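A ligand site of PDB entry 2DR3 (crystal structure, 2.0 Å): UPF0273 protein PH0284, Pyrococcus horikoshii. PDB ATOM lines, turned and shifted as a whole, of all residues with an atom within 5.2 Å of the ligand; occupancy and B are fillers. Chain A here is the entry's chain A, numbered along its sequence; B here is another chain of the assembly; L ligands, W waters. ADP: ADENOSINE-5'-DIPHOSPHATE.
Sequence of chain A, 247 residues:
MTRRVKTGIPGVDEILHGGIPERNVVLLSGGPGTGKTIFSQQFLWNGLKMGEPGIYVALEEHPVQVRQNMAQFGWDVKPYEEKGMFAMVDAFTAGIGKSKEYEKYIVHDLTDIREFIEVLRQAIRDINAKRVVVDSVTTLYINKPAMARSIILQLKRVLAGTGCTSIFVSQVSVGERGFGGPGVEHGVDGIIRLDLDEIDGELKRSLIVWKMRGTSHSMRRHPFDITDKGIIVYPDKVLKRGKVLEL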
ATOM      1  N   GLY A  31      -4.798   4.473 -15.724  1.00  0.00           N
ATOM      2  CA  GLY A  31      -3.814   5.373 -16.287  1.00  0.00           C
ATOM      3  C   GLY A  31      -4.203   6.830 -16.124  1.00  0.00           C
ATOM      4  O   GLY A  31      -5.254   7.142 -15.544  1.00  0.00           O
ATOM      5  N   PRO A  32      -3.382   7.750 -16.624  1.00  0.00           N
ATOM      6  CA  PRO A  32      -3.705   9.164 -16.497  1.00  0.00           C
ATOM      7  C   PRO A  32      -4.966   9.539 -17.251  1.00  0.00           C
ATOM      8  O   PRO A  32      -5.228   9.014 -18.337  1.00  0.00           O
ATOM      9  CB  PRO A  32      -2.467   9.858 -17.085  1.00  0.00           C
ATOM     10  CG  PRO A  32      -2.000   8.891 -18.101  1.00  0.00           C
ATOM     11  CD  PRO A  32      -2.123   7.570 -17.386  1.00  0.00           C
ATOM     12  N   GLY A  33      -5.752  10.434 -16.650  1.00  0.00           N
ATOM     13  CA  GLY A  33      -6.971  10.920 -17.278  1.00  0.00           C
ATOM     14  C   GLY A  33      -8.098   9.909 -17.376  1.00  0.00           C
ATOM     15  O   GLY A  33      -8.973  10.036 -18.242  1.00  0.00           O
ATOM     16  N   THR A  34      -8.109   8.904 -16.511  1.00  0.00           N
ATOM     17  CA  THR A  34      -9.185   7.926 -16.561  1.00  0.00           C
ATOM     18  C   THR A  34     -10.335   8.283 -15.627  1.00  0.00           C
ATOM     19  O   THR A  34     -11.381   7.645 -15.643  1.00  0.00           O
ATOM     20  CB  THR A  34      -8.667   6.510 -16.218  1.00  0.00           C
ATOM     21  OG1 THR A  34      -7.894   6.564 -15.011  1.00  0.00           O
ATOM     22  CG2 THR A  34      -7.813   5.986 -17.346  1.00  0.00           C
ATOM     23  N   GLY A  35     -10.135   9.315 -14.799  1.00  0.00           N
ATOM     24  CA  GLY A  35     -11.191   9.746 -13.891  1.00  0.00           C
ATOM     25  C   GLY A  35     -11.046   9.370 -12.429  1.00  0.00           C
ATOM     26  O   GLY A  35     -11.971   9.607 -11.634  1.00  0.00           O
ATOM     27  N   LYS A  36      -9.908   8.799 -12.057  1.00  0.00           N
ATOM     28  CA  LYS A  36      -9.690   8.379 -10.683  1.00  0.00           C
ATOM     29  C   LYS A  36      -9.827   9.513  -9.674  1.00  0.00           C
ATOM     30  O   LYS A  36     -10.323   9.314  -8.566  1.00  0.00           O
ATOM     31  CB  LYS A  36      -8.292   7.742 -10.542  1.00  0.00           C
ATOM     32  CG  LYS A  36      -8.021   6.619 -11.530  1.00  0.00           C
ATOM     33  CD  LYS A  36      -6.639   5.985 -11.302  1.00  0.00           C
ATOM     34  CE  LYS A  36      -5.512   7.011 -11.417  1.00  0.00           C
ATOM     35  NZ  LYS A  36      -5.406   7.575 -12.795  1.00  0.00           N
ATOM     36  N   THR A  37      -9.398  10.711 -10.056  1.00  0.00           N
ATOM     37  CA  THR A  37      -9.481  11.864  -9.160  1.00  0.00           C
ATOM     38  C   THR A  37     -10.915  12.331  -8.949  1.00  0.00           C
ATOM     39  O   THR A  37     -11.366  12.509  -7.821  1.00  0.00           O
ATOM     40  CB  THR A  37      -8.628  13.039  -9.668  1.00  0.00           C
ATOM     41  OG1 THR A  37      -7.238  12.707  -9.512  1.00  0.00           O
ATOM     42  CG2 THR A  37      -8.926  14.315  -8.884  1.00  0.00           C
ATOM     43  N   ILE A  38     -11.630  12.538 -10.049  1.00  0.00           N
ATOM     44  CA  ILE A  38     -13.015  12.974  -9.958  1.00  0.00           C
ATOM     45  C   ILE A  38     -13.833  11.910  -9.217  1.00  0.00           C
ATOM     46  O   ILE A  38     -14.662  12.248  -8.364  1.00  0.00           O
ATOM     47  CB  ILE A  38     -13.610  13.214 -11.363  1.00  0.00           C
ATOM     48  CG1 ILE A  38     -12.793  14.285 -12.088  1.00  0.00           C
ATOM     49  CG2 ILE A  38     -15.079  13.641 -11.258  1.00  0.00           C
ATOM     50  CD1 ILE A  38     -13.151  14.455 -13.545  1.00  0.00           C
ATOM     51  N   PHE A  39     -13.578  10.639  -9.533  1.00  0.00           N
ATOM     52  CA  PHE A  39     -14.276   9.513  -8.898  1.00  0.00           C
ATOM     53  C   PHE A  39     -14.137   9.477  -7.380  1.00  0.00           C
ATOM     54  O   PHE A  39     -15.143   9.383  -6.667  1.00  0.00           O
ATOM     55  CB  PHE A  39     -13.763   8.193  -9.486  1.00  0.00           C
ATOM     56  CG  PHE A  39     -14.468   6.958  -8.954  1.00  0.00           C
ATOM     57  CD1 PHE A  39     -14.285   6.543  -7.643  1.00  0.00           C
ATOM     58  CD2 PHE A  39     -15.306   6.220  -9.786  1.00  0.00           C
ATOM     59  CE1 PHE A  39     -14.926   5.392  -7.164  1.00  0.00           C
ATOM     60  CE2 PHE A  39     -15.946   5.071  -9.321  1.00  0.00           C
ATOM     61  CZ  PHE A  39     -15.756   4.656  -8.002  1.00  0.00           C
ATOM     62  N   PHE A  73     -16.942  21.341  -9.762  1.00  0.00           N
ATOM     63  CA  PHE A  73     -17.957  20.323 -10.057  1.00  0.00           C
ATOM     64  C   PHE A  73     -19.193  20.609  -9.220  1.00  0.00           C
ATOM     65  O   PHE A  73     -20.176  19.864  -9.269  1.00  0.00           O
ATOM     66  CB  PHE A  73     -17.434  18.920  -9.719  1.00  0.00           C
ATOM     67  CG  PHE A  73     -16.478  18.376 -10.738  1.00  0.00           C
ATOM     68  CD1 PHE A  73     -16.932  17.966 -11.988  1.00  0.00           C
ATOM     69  CD2 PHE A  73     -15.120  18.251 -10.439  1.00  0.00           C
ATOM     70  CE1 PHE A  73     -16.052  17.436 -12.931  1.00  0.00           C
ATOM     71  CE2 PHE A  73     -14.235  17.730 -11.374  1.00  0.00           C
ATOM     72  CZ  PHE A  73     -14.703  17.318 -12.624  1.00  0.00           C
ATOM     73  N   ARG A 205     -14.526   5.286 -22.187  1.00  0.00           N
ATOM     74  CA  ARG A 205     -14.256   5.088 -20.784  1.00  0.00           C
ATOM     75  C   ARG A 205     -15.028   3.867 -20.285  1.00  0.00           C
ATOM     76  O   ARG A 205     -16.165   3.631 -20.698  1.00  0.00           O
ATOM     77  CB  ARG A 205     -14.695   6.311 -19.970  1.00  0.00           C
ATOM     78  CG  ARG A 205     -14.029   7.626 -20.351  1.00  0.00           C
ATOM     79  CD  ARG A 205     -14.433   8.727 -19.386  1.00  0.00           C
ATOM     80  NE  ARG A 205     -13.858  10.027 -19.718  1.00  0.00           N
ATOM     81  CZ  ARG A 205     -12.578  10.329 -19.591  1.00  0.00           C
ATOM     82  NH1 ARG A 205     -11.718   9.425 -19.147  1.00  0.00           N
ATOM     83  NH2 ARG A 205     -12.147  11.549 -19.919  1.00  0.00           N
ATOM     84  N   ILE A 226     -17.702  11.118 -17.954  1.00  0.00           N
ATOM     85  CA  ILE A 226     -17.326  12.078 -16.933  1.00  0.00           C
ATOM     86  C   ILE A 226     -18.105  13.317 -17.379  1.00  0.00           C
ATOM     87  O   ILE A 226     -18.062  13.671 -18.562  1.00  0.00           O
ATOM     88  CB  ILE A 226     -15.801  12.387 -16.938  1.00  0.00           C
ATOM     89  CG1 ILE A 226     -15.011  11.130 -16.502  1.00  0.00           C
ATOM     90  CG2 ILE A 226     -15.494  13.532 -15.993  1.00  0.00           C
ATOM     91  CD1 ILE A 226     -13.526  11.376 -16.424  1.00  0.00           C
ATOM     92  N   THR A 227     -18.844  13.941 -16.466  1.00  0.00           N
ATOM     93  CA  THR A 227     -19.640  15.113 -16.837  1.00  0.00           C
ATOM     94  C   THR A 227     -19.401  16.277 -15.895  1.00  0.00           C
ATOM     95  O   THR A 227     -18.631  16.169 -14.952  1.00  0.00           O
ATOM     96  CB  THR A 227     -21.159  14.809 -16.796  1.00  0.00           C
ATOM     97  OG1 THR A 227     -21.536  14.460 -15.463  1.00  0.00           O
ATOM     98  CG2 THR A 227     -21.501  13.656 -17.735  1.00  0.00           C
ATOM     99  N   ASP A 228     -20.080  17.392 -16.170  1.00  0.00           N
ATOM    100  CA  ASP A 228     -19.971  18.605 -15.354  1.00  0.00           C
ATOM    101  C   ASP A 228     -20.303  18.316 -13.898  1.00  0.00           C
ATOM    102  O   ASP A 228     -19.844  19.034 -12.998  1.00  0.00           O
ATOM    103  CB  ASP A 228     -20.929  19.687 -15.859  1.00  0.00           C
ATOM    104  CG  ASP A 228     -20.502  20.269 -17.175  1.00  0.00           C
ATOM    105  OD1 ASP A 228     -19.298  20.573 -17.325  1.00  0.00           O
ATOM    106  OD2 ASP A 228     -21.367  20.454 -18.068  1.00  0.00           O
ATOM    107  N   TRP B 210      -5.785  13.182 -24.781  1.00  0.00           N
ATOM    108  CA  TRP B 210      -5.931  12.088 -23.849  1.00  0.00           C
ATOM    109  C   TRP B 210      -6.441  12.567 -22.498  1.00  0.00           C
ATOM    110  O   TRP B 210      -7.151  11.851 -21.802  1.00  0.00           O
ATOM    111  CB  TRP B 210      -4.586  11.380 -23.655  1.00  0.00           C
ATOM    112  CG  TRP B 210      -4.732   9.909 -23.481  1.00  0.00           C
ATOM    113  CD1 TRP B 210      -4.939   9.239 -22.313  1.00  0.00           C
ATOM    114  CD2 TRP B 210      -4.790   8.941 -24.523  1.00  0.00           C
ATOM    115  NE1 TRP B 210      -5.124   7.896 -22.569  1.00  0.00           N
ATOM    116  CE2 TRP B 210      -5.032   7.688 -23.917  1.00  0.00           C
ATOM    117  CE3 TRP B 210      -4.646   8.998 -25.914  1.00  0.00           C
ATOM    118  CZ2 TRP B 210      -5.149   6.512 -24.655  1.00  0.00           C
ATOM    119  CZ3 TRP B 210      -4.756   7.822 -26.646  1.00  0.00           C
ATOM    120  CH2 TRP B 210      -5.010   6.594 -26.014  1.00  0.00           C
ATOM    121  N   LYS B 211      -6.083  13.791 -22.143  1.00  0.00           N
ATOM    122  CA  LYS B 211      -6.452  14.328 -20.850  1.00  0.00           C
ATOM    123  C   LYS B 211      -6.439  15.846 -20.848  1.00  0.00           C
ATOM    124  O   LYS B 211      -5.594  16.487 -21.495  1.00  0.00           O
ATOM    125  CB  LYS B 211      -5.454  13.803 -19.815  1.00  0.00           C
ATOM    126  CG  LYS B 211      -5.549  14.373 -18.414  1.00  0.00           C
ATOM    127  CD  LYS B 211      -4.387  13.829 -17.572  1.00  0.00           C
ATOM    128  CE  LYS B 211      -4.333  14.451 -16.193  1.00  0.00           C
ATOM    129  NZ  LYS B 211      -3.067  14.054 -15.487  1.00  0.00           N
ATOM    130  N   MET B 212      -7.399  16.432 -20.138  1.00  0.00           N
ATOM    131  CA  MET B 212      -7.454  17.875 -20.012  1.00  0.00           C
ATOM    132  C   MET B 212      -8.348  18.232 -18.853  1.00  0.00           C
ATOM    133  O   MET B 212      -9.563  18.317 -18.996  1.00  0.00           O
ATOM    134  CB  MET B 212      -7.978  18.539 -21.282  1.00  0.00           C
ATOM    135  CG  MET B 212      -7.734  20.049 -21.272  1.00  0.00           C
ATOM    136  SD  MET B 212      -5.944  20.473 -21.177  1.00  0.00           S
ATOM    137  CE  MET B 212      -5.447  19.999 -22.756  1.00  0.00           C
ATOM    138  N   ARG B 213      -7.738  18.427 -17.685  1.00  0.00           N
ATOM    139  CA  ARG B 213      -8.481  18.786 -16.493  1.00  0.00           C
ATOM    140  C   ARG B 213      -9.233  20.093 -16.699  1.00  0.00           C
ATOM    141  O   ARG B 213      -8.725  21.004 -17.367  1.00  0.00           O
ATOM    142  CB  ARG B 213      -7.532  18.939 -15.309  1.00  0.00           C
ATOM    143  CG  ARG B 213      -6.961  17.613 -14.823  1.00  0.00           C
ATOM    144  CD  ARG B 213      -5.868  17.815 -13.770  1.00  0.00           C
ATOM    145  NE  ARG B 213      -5.249  16.547 -13.390  1.00  0.00           N
ATOM    146  CZ  ARG B 213      -4.116  16.444 -12.682  1.00  0.00           C
ATOM    147  NH1 ARG B 213      -3.468  17.531 -12.291  1.00  0.00           N
ATOM    148  NH2 ARG B 213      -3.638  15.246 -12.388  1.00  0.00           N
ATOM    149  N   GLY B 214     -10.447  20.165 -16.163  1.00  0.00           N
ATOM    150  CA  GLY B 214     -11.239  21.376 -16.270  1.00  0.00           C
ATOM    151  C   GLY B 214     -12.110  21.575 -17.497  1.00  0.00           C
ATOM    152  O   GLY B 214     -12.635  22.673 -17.685  1.00  0.00           O
ATOM    153  N   THR B 215     -12.289  20.546 -18.318  1.00  0.00           N
ATOM    154  CA  THR B 215     -13.105  20.688 -19.512  1.00  0.00           C
ATOM    155  C   THR B 215     -13.334  19.380 -20.264  1.00  0.00           C
ATOM    156  O   THR B 215     -12.550  18.444 -20.140  1.00  0.00           O
ATOM    157  CB  THR B 215     -12.463  21.670 -20.515  1.00  0.00           C
ATOM    158  OG1 THR B 215     -13.294  21.774 -21.680  1.00  0.00           O
ATOM    159  CG2 THR B 215     -11.076  21.169 -20.946  1.00  0.00           C
ATOM    160  N   SER B 216     -14.417  19.337 -21.033  1.00  0.00           N
ATOM    161  CA  SER B 216     -14.716  18.181 -21.843  1.00  0.00           C
ATOM    162  C   SER B 216     -13.919  18.503 -23.102  1.00  0.00           C
ATOM    163  O   SER B 216     -13.436  19.631 -23.253  1.00  0.00           O
ATOM    164  CB  SER B 216     -16.217  18.110 -22.179  1.00  0.00           C
ATOM    165  OG  SER B 216     -16.692  19.345 -22.689  1.00  0.00           O
ATOM    166  N   HIS B 217     -13.784  17.533 -23.983  1.00  0.00           N
ATOM    167  CA  HIS B 217     -13.026  17.720 -25.213  1.00  0.00           C
ATOM    168  C   HIS B 217     -13.340  16.567 -26.123  1.00  0.00           C
ATOM    169  O   HIS B 217     -13.940  15.588 -25.702  1.00  0.00           O
ATOM    170  CB  HIS B 217     -11.515  17.735 -24.901  1.00  0.00           C
ATOM    171  CG  HIS B 217     -11.072  16.606 -24.022  1.00  0.00           C
ATOM    172  ND1 HIS B 217     -10.719  15.363 -24.507  1.00  0.00           N
ATOM    173  CD2 HIS B 217     -10.960  16.532 -22.674  1.00  0.00           C
ATOM    174  CE1 HIS B 217     -10.404  14.568 -23.491  1.00  0.00           C
ATOM    175  NE2 HIS B 217     -10.546  15.249 -22.371  1.00  0.00           N
ATOM    176  N   MET B 219     -13.098  13.199 -28.015  1.00  0.00           N
ATOM    177  CA  MET B 219     -12.515  11.931 -27.613  1.00  0.00           C
ATOM    178  C   MET B 219     -12.084  11.172 -28.865  1.00  0.00           C
ATOM    179  O   MET B 219     -11.784   9.981 -28.804  1.00  0.00           O
ATOM    180  CB  MET B 219     -13.542  11.100 -26.836  1.00  0.00           C
ATOM    181  CG  MET B 219     -14.092  11.765 -25.590  1.00  0.00           C
ATOM    182  SD  MET B 219     -12.889  11.895 -24.235  1.00  0.00           S
ATOM    183  CE  MET B 219     -13.348  10.468 -23.267  1.00  0.00           C
HETATM  184  PB  ADP L   1      -7.011  10.986 -13.402  1.00  0.00           P
HETATM  185  O1B ADP L   1      -7.392   9.562 -13.518  1.00  0.00           O
HETATM  186  O2B ADP L   1      -5.578  11.255 -14.064  1.00  0.00           O
HETATM  187  O3B ADP L   1      -6.903  11.418 -11.877  1.00  0.00           O
HETATM  188  PA  ADP L   1      -9.178  12.855 -13.503  1.00  0.00           P
HETATM  189  O1A ADP L   1      -9.855  12.020 -12.497  1.00  0.00           O
HETATM  190  O2A ADP L   1      -8.563  14.119 -13.039  1.00  0.00           O
HETATM  191  O3A ADP L   1      -7.988  11.995 -14.170  1.00  0.00           O
HETATM  192  O5' ADP L   1     -10.121  13.177 -14.745  1.00  0.00           O
HETATM  193  C5' ADP L   1      -9.681  14.091 -15.754  1.00  0.00           C
HETATM  194  C4' ADP L   1     -10.601  14.092 -16.957  1.00  0.00           C
HETATM  195  O4' ADP L   1     -11.927  14.544 -16.599  1.00  0.00           O
HETATM  196  C3' ADP L   1     -10.149  15.059 -18.023  1.00  0.00           C
HETATM  197  O3' ADP L   1      -9.082  14.482 -18.783  1.00  0.00           O
HETATM  198  C2' ADP L   1     -11.420  15.257 -18.834  1.00  0.00           C
HETATM  199  O2' ADP L   1     -11.443  14.419 -19.998  1.00  0.00           O
HETATM  200  C1' ADP L   1     -12.552  14.897 -17.848  1.00  0.00           C
HETATM  201  N9  ADP L   1     -13.456  16.067 -17.601  1.00  0.00           N
HETATM  202  C8  ADP L   1     -13.204  17.085 -16.755  1.00  0.00           C
HETATM  203  N7  ADP L   1     -14.218  17.939 -16.774  1.00  0.00           N
HETATM  204  C5  ADP L   1     -15.120  17.474 -17.645  1.00  0.00           C
HETATM  205  C6  ADP L   1     -16.384  17.917 -18.072  1.00  0.00           C
HETATM  206  N6  ADP L   1     -16.890  19.054 -17.615  1.00  0.00           N
HETATM  207  N1  ADP L   1     -17.061  17.174 -19.007  1.00  0.00           N
HETATM  208  C2  ADP L   1     -16.568  16.027 -19.480  1.00  0.00           C
HETATM  209  N3  ADP L   1     -15.368  15.578 -19.089  1.00  0.00           N
HETATM  210  C4  ADP L   1     -14.645  16.267 -18.156  1.00  0.00           C
HETATM  211  O   HOH W   1      -9.319  12.011 -19.929  1.00  0.00           O
HETATM  212  O   HOH W   2     -14.681  13.300 -20.527  1.00  0.00           O
HETATM  213  O   HOH W   3      -9.629  16.349 -12.225  1.00  0.00           O
HETATM  214  O   HOH W   4     -14.318  20.133 -15.102  1.00  0.00           O
HETATM  215  O   HOH W   5     -19.409  17.653 -20.118  1.00  0.00           O
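An oxygen (O2') of the ligand lies within hydrogen-bond range of a ring nitrogen (NE2) of His 217 of chain B. N of Thr 37 is in hydrogen-bond range of O1A of the ligand (2.8 Å). The side-chain hydroxyl (OG1) of Thr 37 lies within hydrogen-bond range of an oxygen (O3B) of the ligand, 2.7 Å away. N of Gly 33 sits at hydrogen-bond distance from O2B of the ligand (2.7 Å). The side-chain carboxylate of Asp 228 sits at hydrogen-bond distance from a nitrogen (N6) of the ligand (2.9 Å). N of Lys 36 lies within hydrogen-bond range of O1B of the ligand, at 3.0 Å. The side-chain amino group (NZ) of Lys 36 is in salt-bridge range of an oxygen (O1B) of the ligand (2.9 Å). The backbone NH (N) of Gly 35 is in hydrogen-bond range of an oxygen (O1B) of the ligand (3.0 Å). The backbone NH (N) of Met 212 of chain B is in hydrogen-bond range of an oxygen (O3') of the ligand (2.9 Å). The guanidinium group (NH2) of Arg 205 is in hydrogen-bond range of an oxygen (O2') of the ligand (3.0 Å). N of Ile 38 sits at hydrogen-bond distance from O1A of the ligand, 3.1 Å away. The backbone NH (N) of Thr 34 lies within hydrogen-bond range of an oxygen (O1B) of the ligand. The side-chain hydroxyl of Thr 34 is in hydrogen-bond range of an oxygen (O1B) of the ligand (3.4 Å).
The backbone carbonyl oxygen (O) of Ile 226 lies close to a nitrogen (N3) of the ligand (3.3 Å). Gly 31 touches the ligand. Pro 32 touches the ligand (C to O2B, 3.7 Å). Thr 227 touches the ligand (CA to N1, 3.95 Å). CA of Lys 211 of chain B touches O3' of the ligand, at 3.3 Å. Thr 215 of chain B touches the ligand. Ser 216 of chain B touches the ligand (CB to N1, 3.4 Å). Within 4 Å of the ligand: Gly 31, Pro 32, Gly 33, Thr 34, Gly 35, Lys 36, Thr 37, Ile 38, Arg 205, Ile 226, Thr 227, Asp 228, Lys 211 of chain B, Met 212 of chain B, Thr 215 of chain B, Ser 216 of chain B and His 217 of chain B. Along chain A the residues within 4 Å of the ligand span positions 31 to 228. The nearest printed residue that does not touch the ligand is Arg 213 of chain B (4.1 Å).
The guanidinium group of Arg 205 sits at hydrogen-bond distance from the backbone carbonyl oxygen of Gly 33, at 3.0 Å. The side-chain hydroxyl (OG1) of Thr 34 is in hydrogen-bond range of the side-chain amino group (NZ) of Lys 36, 3.5 Å away. O of Gly 31 is in hydrogen-bond range of NZ of Lys 36 (2.8 Å). OG1 of Thr 34 sits at hydrogen-bond distance from O of Gly 31 (2.8 Å).
Water W1 lies within hydrogen-bond range of O of Gly 33, O3' of the ligand, NH2 of Arg 205 and O of Trp 210 of chain B. Water W2 bridges N3 of the ligand and NH2 of Arg 205.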
